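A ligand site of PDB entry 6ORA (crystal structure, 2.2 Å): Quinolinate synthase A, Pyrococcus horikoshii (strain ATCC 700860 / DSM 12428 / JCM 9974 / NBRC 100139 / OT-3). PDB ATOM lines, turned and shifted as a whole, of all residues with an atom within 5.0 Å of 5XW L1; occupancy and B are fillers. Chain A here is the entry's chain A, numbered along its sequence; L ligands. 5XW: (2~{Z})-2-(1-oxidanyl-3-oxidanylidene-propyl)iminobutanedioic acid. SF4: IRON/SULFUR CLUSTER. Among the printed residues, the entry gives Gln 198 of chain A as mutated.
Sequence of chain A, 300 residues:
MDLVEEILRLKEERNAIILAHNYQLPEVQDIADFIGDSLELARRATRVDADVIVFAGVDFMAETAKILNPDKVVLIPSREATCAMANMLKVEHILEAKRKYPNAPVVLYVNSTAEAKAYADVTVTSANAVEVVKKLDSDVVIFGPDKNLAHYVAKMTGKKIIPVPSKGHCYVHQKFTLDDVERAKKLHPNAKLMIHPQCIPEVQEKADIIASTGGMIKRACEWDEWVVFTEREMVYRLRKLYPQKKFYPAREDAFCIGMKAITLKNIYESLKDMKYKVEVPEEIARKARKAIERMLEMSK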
ATOM      1  N   HIS A  21      21.371  11.008  25.803  1.00  0.00           N
ATOM      2  CA  HIS A  21      20.939   9.719  26.333  1.00  0.00           C
ATOM      3  C   HIS A  21      21.953   9.212  27.348  1.00  0.00           C
ATOM      4  O   HIS A  21      23.115   9.632  27.366  1.00  0.00           O
ATOM      5  CB  HIS A  21      20.752   8.705  25.203  1.00  0.00           C
ATOM      6  CG  HIS A  21      20.198   7.398  25.648  1.00  0.00           C
ATOM      7  ND1 HIS A  21      20.978   6.253  25.754  1.00  0.00           N
ATOM      8  CD2 HIS A  21      18.957   7.039  26.038  1.00  0.00           C
ATOM      9  CE1 HIS A  21      20.226   5.253  26.181  1.00  0.00           C
ATOM     10  NE2 HIS A  21      18.998   5.701  26.362  1.00  0.00           N
ATOM     11  N   TYR A  23      23.536   6.602  27.408  1.00  0.00           N
ATOM     12  CA  TYR A  23      24.650   5.908  26.792  1.00  0.00           C
ATOM     13  C   TYR A  23      25.688   6.851  26.199  1.00  0.00           C
ATOM     14  O   TYR A  23      26.635   6.377  25.555  1.00  0.00           O
ATOM     15  CB  TYR A  23      24.155   4.949  25.700  1.00  0.00           C
ATOM     16  CG  TYR A  23      23.272   3.815  26.194  1.00  0.00           C
ATOM     17  CD1 TYR A  23      23.160   3.527  27.552  1.00  0.00           C
ATOM     18  CD2 TYR A  23      22.563   3.032  25.292  1.00  0.00           C
ATOM     19  CE1 TYR A  23      22.357   2.490  27.997  1.00  0.00           C
ATOM     20  CE2 TYR A  23      21.757   1.993  25.724  1.00  0.00           C
ATOM     21  CZ  TYR A  23      21.658   1.731  27.074  1.00  0.00           C
ATOM     22  OH  TYR A  23      20.855   0.694  27.520  1.00  0.00           O
ATOM     23  N   ASP A  37      16.457   8.323  29.715  1.00  0.00           N
ATOM     24  CA  ASP A  37      16.213   7.259  28.760  1.00  0.00           C
ATOM     25  C   ASP A  37      15.311   7.774  27.651  1.00  0.00           C
ATOM     26  O   ASP A  37      14.964   8.960  27.587  1.00  0.00           O
ATOM     27  CB  ASP A  37      15.646   6.016  29.457  1.00  0.00           C
ATOM     28  CG  ASP A  37      14.253   6.217  30.031  1.00  0.00           C
ATOM     29  OD1 ASP A  37      13.614   7.267  29.764  1.00  0.00           O
ATOM     30  OD2 ASP A  37      13.781   5.318  30.764  1.00  0.00           O
ATOM     31  N   SER A  38      14.900   6.861  26.760  1.00  0.00           N
ATOM     32  CA  SER A  38      14.172   7.272  25.564  1.00  0.00           C
ATOM     33  C   SER A  38      12.804   7.848  25.900  1.00  0.00           C
ATOM     34  O   SER A  38      12.341   8.775  25.225  1.00  0.00           O
ATOM     35  CB  SER A  38      14.048   6.094  24.589  1.00  0.00           C
ATOM     36  OG  SER A  38      12.811   6.137  23.918  1.00  0.00           O
ATOM     37  N   LEU A  39      12.148   7.308  26.914  1.00  0.00           N
ATOM     38  CA  LEU A  39      10.844   7.846  27.321  1.00  0.00           C
ATOM     39  C   LEU A  39      10.994   9.223  27.966  1.00  0.00           C
ATOM     40  O   LEU A  39      10.243  10.146  27.657  1.00  0.00           O
ATOM     41  CB  LEU A  39      10.152   6.869  28.282  1.00  0.00           C
ATOM     42  CG  LEU A  39       8.869   7.409  28.904  1.00  0.00           C
ATOM     43  CD1 LEU A  39       7.886   7.832  27.813  1.00  0.00           C
ATOM     44  CD2 LEU A  39       8.244   6.387  29.826  1.00  0.00           C
ATOM     45  N   PHE A  60      16.991   7.759  15.546  1.00  0.00           N
ATOM     46  CA  PHE A  60      15.565   7.602  15.856  1.00  0.00           C
ATOM     47  C   PHE A  60      15.172   8.460  17.043  1.00  0.00           C
ATOM     48  O   PHE A  60      14.005   8.877  17.146  1.00  0.00           O
ATOM     49  CB  PHE A  60      15.223   6.125  16.082  1.00  0.00           C
ATOM     50  CG  PHE A  60      15.573   5.588  17.457  1.00  0.00           C
ATOM     51  CD1 PHE A  60      14.744   5.822  18.548  1.00  0.00           C
ATOM     52  CD2 PHE A  60      16.703   4.818  17.649  1.00  0.00           C
ATOM     53  CE1 PHE A  60      15.052   5.334  19.808  1.00  0.00           C
ATOM     54  CE2 PHE A  60      17.019   4.301  18.904  1.00  0.00           C
ATOM     55  CZ  PHE A  60      16.201   4.572  19.980  1.00  0.00           C
ATOM     56  N   MET A  61      16.105   8.723  17.958  1.00  0.00           N
ATOM     57  CA  MET A  61      15.798   9.602  19.091  1.00  0.00           C
ATOM     58  C   MET A  61      15.640  11.046  18.640  1.00  0.00           C
ATOM     59  O   MET A  61      14.724  11.744  19.097  1.00  0.00           O
ATOM     60  CB  MET A  61      16.899   9.481  20.152  1.00  0.00           C
ATOM     61  CG  MET A  61      16.937   8.151  20.880  1.00  0.00           C
ATOM     62  SD  MET A  61      18.263   8.061  22.103  1.00  0.00           S
ATOM     63  CE  MET A  61      18.002   6.427  22.758  1.00  0.00           C
ATOM     64  N   MET A  85      19.455  -2.028  15.976  1.00  0.00           N
ATOM     65  CA  MET A  85      18.225  -2.799  16.158  1.00  0.00           C
ATOM     66  C   MET A  85      17.055  -2.137  15.454  1.00  0.00           C
ATOM     67  O   MET A  85      16.222  -2.821  14.848  1.00  0.00           O
ATOM     68  CB  MET A  85      17.933  -2.980  17.647  1.00  0.00           C
ATOM     69  CG  MET A  85      16.668  -3.772  17.936  1.00  0.00           C
ATOM     70  SD  MET A  85      15.306  -2.714  18.436  1.00  0.00           S
ATOM     71  CE  MET A  85      15.999  -2.015  19.928  1.00  0.00           C
ATOM     72  N   TYR A 109       8.501  -0.481  19.195  1.00  0.00           N
ATOM     73  CA  TYR A 109       9.559   0.137  19.991  1.00  0.00           C
ATOM     74  C   TYR A 109       9.909   1.502  19.411  1.00  0.00           C
ATOM     75  O   TYR A 109       9.916   1.696  18.189  1.00  0.00           O
ATOM     76  CB  TYR A 109      10.787  -0.776  19.974  1.00  0.00           C
ATOM     77  CG  TYR A 109      11.642  -0.821  21.225  1.00  0.00           C
ATOM     78  CD1 TYR A 109      11.375  -0.007  22.328  1.00  0.00           C
ATOM     79  CD2 TYR A 109      12.726  -1.687  21.318  1.00  0.00           C
ATOM     80  CE1 TYR A 109      12.163  -0.048  23.463  1.00  0.00           C
ATOM     81  CE2 TYR A 109      13.518  -1.747  22.439  1.00  0.00           C
ATOM     82  CZ  TYR A 109      13.233  -0.929  23.517  1.00  0.00           C
ATOM     83  OH  TYR A 109      14.033  -0.991  24.644  1.00  0.00           O
ATOM     84  N   ASN A 111      12.725   2.657  19.251  1.00  0.00           N
ATOM     85  CA  ASN A 111      13.840   2.312  18.385  1.00  0.00           C
ATOM     86  C   ASN A 111      13.278   1.792  17.070  1.00  0.00           C
ATOM     87  O   ASN A 111      13.159   0.581  16.834  1.00  0.00           O
ATOM     88  CB  ASN A 111      14.747   1.275  19.039  1.00  0.00           C
ATOM     89  CG  ASN A 111      15.037   1.580  20.490  1.00  0.00           C
ATOM     90  OD1 ASN A 111      14.144   1.987  21.241  1.00  0.00           O
ATOM     91  ND2 ASN A 111      16.289   1.396  20.891  1.00  0.00           N
ATOM     92  N   THR A 125       8.445   2.378  24.841  1.00  0.00           N
ATOM     93  CA  THR A 125       9.823   2.360  25.282  1.00  0.00           C
ATOM     94  C   THR A 125       9.996   1.173  26.235  1.00  0.00           C
ATOM     95  O   THR A 125       9.047   0.467  26.551  1.00  0.00           O
ATOM     96  CB  THR A 125      10.206   3.680  25.951  1.00  0.00           C
ATOM     97  OG1 THR A 125       9.559   3.776  27.223  1.00  0.00           O
ATOM     98  CG2 THR A 125       9.823   4.849  25.081  1.00  0.00           C
ATOM     99  N   SER A 126      11.243   0.963  26.700  1.00  0.00           N
ATOM    100  CA  SER A 126      11.489  -0.111  27.656  1.00  0.00           C
ATOM    101  C   SER A 126      10.787   0.133  28.979  1.00  0.00           C
ATOM    102  O   SER A 126      10.462  -0.843  29.672  1.00  0.00           O
ATOM    103  CB  SER A 126      12.991  -0.278  27.919  1.00  0.00           C
ATOM    104  OG  SER A 126      13.757  -0.048  26.746  1.00  0.00           O
ATOM    105  N   ALA A 127      10.531   1.387  29.338  1.00  0.00           N
ATOM    106  CA  ALA A 127       9.950   1.690  30.645  1.00  0.00           C
ATOM    107  C   ALA A 127       8.430   1.539  30.668  1.00  0.00           C
ATOM    108  O   ALA A 127       7.854   1.298  31.737  1.00  0.00           O
ATOM    109  CB  ALA A 127      10.331   3.105  31.066  1.00  0.00           C
ATOM    110  N   HIS A 173      23.219  -5.540  23.831  1.00  0.00           N
ATOM    111  CA  HIS A 173      22.637  -6.253  24.947  1.00  0.00           C
ATOM    112  C   HIS A 173      22.685  -7.766  24.773  1.00  0.00           C
ATOM    113  O   HIS A 173      22.637  -8.488  25.772  1.00  0.00           O
ATOM    114  CB  HIS A 173      21.190  -5.797  25.166  1.00  0.00           C
ATOM    115  CG  HIS A 173      21.088  -4.436  25.780  1.00  0.00           C
ATOM    116  ND1 HIS A 173      21.045  -3.276  25.019  1.00  0.00           N
ATOM    117  CD2 HIS A 173      21.050  -4.038  27.071  1.00  0.00           C
ATOM    118  CE1 HIS A 173      20.966  -2.234  25.829  1.00  0.00           C
ATOM    119  NE2 HIS A 173      20.971  -2.660  27.074  1.00  0.00           N
ATOM    120  N   HIS A 196      18.788  -5.123  31.579  1.00  0.00           N
ATOM    121  CA  HIS A 196      17.914  -4.449  30.638  1.00  0.00           C
ATOM    122  C   HIS A 196      17.036  -5.467  29.915  1.00  0.00           C
ATOM    123  O   HIS A 196      17.479  -6.588  29.637  1.00  0.00           O
ATOM    124  CB  HIS A 196      18.775  -3.667  29.626  1.00  0.00           C
ATOM    125  CG  HIS A 196      18.017  -2.636  28.855  1.00  0.00           C
ATOM    126  ND1 HIS A 196      17.297  -2.921  27.714  1.00  0.00           N
ATOM    127  CD2 HIS A 196      17.889  -1.297  29.045  1.00  0.00           C
ATOM    128  CE1 HIS A 196      16.749  -1.824  27.241  1.00  0.00           C
ATOM    129  NE2 HIS A 196      17.091  -0.819  28.040  1.00  0.00           N
ATOM    130  N   GLN A 198      16.295  -5.747  26.939  1.00  0.00           N
ATOM    131  CA  GLN A 198      16.808  -6.142  25.633  1.00  0.00           C
ATOM    132  C   GLN A 198      17.790  -7.297  25.705  1.00  0.00           C
ATOM    133  O   GLN A 198      18.240  -7.775  24.654  1.00  0.00           O
ATOM    134  CB  GLN A 198      17.475  -4.952  24.934  1.00  0.00           C
ATOM    135  CG  GLN A 198      16.489  -3.911  24.438  1.00  0.00           C
ATOM    136  CD  GLN A 198      17.175  -2.738  23.759  1.00  0.00           C
ATOM    137  OE1 GLN A 198      18.303  -2.854  23.283  1.00  0.00           O
ATOM    138  NE2 GLN A 198      16.497  -1.605  23.718  1.00  0.00           N
ATOM    139  N   SER A 212      14.317  -0.319  32.062  1.00  0.00           N
ATOM    140  CA  SER A 212      15.086   0.582  31.225  1.00  0.00           C
ATOM    141  C   SER A 212      16.137   1.294  32.053  1.00  0.00           C
ATOM    142  O   SER A 212      16.201   1.180  33.282  1.00  0.00           O
ATOM    143  CB  SER A 212      14.171   1.596  30.554  1.00  0.00           C
ATOM    144  OG  SER A 212      13.560   2.424  31.519  1.00  0.00           O
ATOM    145  N   THR A 213      16.999   2.071  31.366  1.00  0.00           N
ATOM    146  CA  THR A 213      18.004   2.836  32.087  1.00  0.00           C
ATOM    147  C   THR A 213      17.364   3.849  33.032  1.00  0.00           C
ATOM    148  O   THR A 213      17.921   4.129  34.097  1.00  0.00           O
ATOM    149  CB  THR A 213      18.954   3.521  31.104  1.00  0.00           C
ATOM    150  OG1 THR A 213      18.231   4.473  30.321  1.00  0.00           O
ATOM    151  CG2 THR A 213      19.601   2.499  30.180  1.00  0.00           C
ATOM    152  N   GLY A 214      16.208   4.396  32.658  1.00  0.00           N
ATOM    153  CA  GLY A 214      15.490   5.248  33.588  1.00  0.00           C
ATOM    154  C   GLY A 214      14.951   4.488  34.781  1.00  0.00           C
ATOM    155  O   GLY A 214      15.015   4.964  35.917  1.00  0.00           O
ATOM    156  N   MET A 259      26.073   5.185  19.393  1.00  0.00           N
ATOM    157  CA  MET A 259      25.975   6.197  20.440  1.00  0.00           C
ATOM    158  C   MET A 259      27.270   6.994  20.562  1.00  0.00           C
ATOM    159  O   MET A 259      27.241   8.203  20.805  1.00  0.00           O
ATOM    160  CB  MET A 259      25.624   5.539  21.770  1.00  0.00           C
ATOM    161  CG  MET A 259      24.161   5.206  21.917  1.00  0.00           C
ATOM    162  SD  MET A 259      23.179   6.632  22.409  1.00  0.00           S
ATOM    163  CE  MET A 259      21.552   5.888  22.479  1.00  0.00           C
HETATM  164  OAD 5XW L   1      17.000   1.117  23.168  1.00  0.00           O
HETATM  165  CAC 5XW L   1      17.767   1.580  24.029  1.00  0.00           C
HETATM  166  OAE 5XW L   1      18.731   2.308  23.736  1.00  0.00           O
HETATM  167  CAA 5XW L   1      17.518   1.227  25.525  1.00  0.00           C
HETATM  168  CAB 5XW L   1      16.474   2.150  26.180  1.00  0.00           C
HETATM  169  CAG 5XW L   1      16.928   2.652  27.598  1.00  0.00           C
HETATM  170  OAI 5XW L   1      17.380   3.812  27.692  1.00  0.00           O
HETATM  171  OAH 5XW L   1      16.789   1.839  28.560  1.00  0.00           O
HETATM  172  NAF 5XW L   1      15.334   2.450  25.609  1.00  0.00           N
HETATM  173  CAJ 5XW L   1      14.241   3.213  25.968  1.00  0.00           C
HETATM  174  OAN 5XW L   1      13.013   2.680  25.540  1.00  0.00           O
HETATM  175  CAK 5XW L   1      14.136   3.587  27.426  1.00  0.00           C
HETATM  176  CAL 5XW L   1      12.972   4.544  27.634  1.00  0.00           C
HETATM  177  OAM 5XW L   1      12.138   4.306  28.479  1.00  0.00           O
HETATM  178 FE1  SF4 L   2      21.312  -1.426  21.064  1.00  0.00          FE
HETATM  179 FE2  SF4 L   2      20.292   1.227  22.182  1.00  0.00          FE
HETATM  180 FE3  SF4 L   2      20.134   0.673  19.152  1.00  0.00          FE
HETATM  181 FE4  SF4 L   2      22.857   1.153  20.453  1.00  0.00          FE
HETATM  182  S1  SF4 L   2      20.973   2.269  20.382  1.00  0.00           S
HETATM  183  S2  SF4 L   2      22.013  -0.451  19.225  1.00  0.00           S
HETATM  184  S3  SF4 L   2      22.199   0.155  22.291  1.00  0.00           S
HETATM  185  S4  SF4 L   2      19.414  -0.350  20.944  1.00  0.00           S
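The side-chain amide nitrogen (ND2) of Asn 111 sits at hydrogen-bond distance from an oxygen (OAD) of 5XW L1, 2.4 Å away.
OAN of 5XW L1 lies within hydrogen-bond range of N of Ser 126 (2.7 Å).
The side-chain hydroxyl (OG) of Ser 126 is in hydrogen-bond range of an oxygen (OAN) of 5XW L1, 3.1 Å away.
A ring nitrogen (NE2) of His 196 is in hydrogen-bond range of an oxygen (OAH) of 5XW L1.
An oxygen (OAI) of 5XW L1 lies within hydrogen-bond range of a ring nitrogen (NE2) of His 21, at 2.8 Å.
An oxygen (OAD) of 5XW L1 sits at hydrogen-bond distance from the side-chain amide nitrogen of Gln 198.
An oxygen (OAH) of 5XW L1 lies within hydrogen-bond range of the backbone NH of Thr 213.
OG1 of Thr 213 lies within hydrogen-bond range of OAI of 5XW L1, at 2.8 Å.
OG1 of Thr 125 is in hydrogen-bond range of OAM of 5XW L1 (2.9 Å).
The backbone NH of Leu 39 lies close to an oxygen (OAM) of 5XW L1 (3.4 Å).
OAM of 5XW L1 lies close to N of Ala 127.
The side-chain amide nitrogen (ND2) of Asn 111 lies close to a sulfur (S4) of SF4 L2.
OE1 of Gln 198 lies close to S4 of SF4 L2.
An oxygen (OAE) of 5XW L1 is bound to an iron atom (FE2) of SF4 L2 (2.5 Å).
The backbone NH of Gln 198 lies close to a ring nitrogen (ND1) of His 196 (3.1 Å).
The backbone NH (N) of Tyr 23 sits close to a ring nitrogen (ND1) of His 21, 3.1 Å away.
The side-chain amide nitrogen (NE2) of Gln 198 sits at hydrogen-bond distance from the side-chain hydroxyl (OH) of Tyr 109 (2.7 Å).
A ring nitrogen (ND1) of His 173 lies within hydrogen-bond range of the side-chain amide oxygen (OE1) of Gln 198.
The backbone NH (N) of Ala 127 sits close to the side-chain hydroxyl (OG1) of Thr 125 (3.3 Å).
OG of Ser 212 is in hydrogen-bond range of OD2 of Asp 37 (3.0 Å).
The side-chain carboxylate of Asp 37 lies within hydrogen-bond range of the backbone NH of Gly 214 (3.2 Å).
OH of Tyr 23 sits close to NE2 of His 173, 3.4 Å away.
An oxygen (OAM) of 5XW L1 sits close to the side-chain carboxylate (OD2) of Asp 37 (3.0 Å).
Residues that only touch 5XW L1: Tyr 23, Ser 38, Tyr 109 and Ser 212.
Hydrophobic or aromatic side chains within 4 Å of 5XW L1: His 21, Tyr 23, Leu 39, Tyr 109, Ala 127 and His 196.
Along chain A the residues within 4 Å of 5XW L1 span positions 21 to 213.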
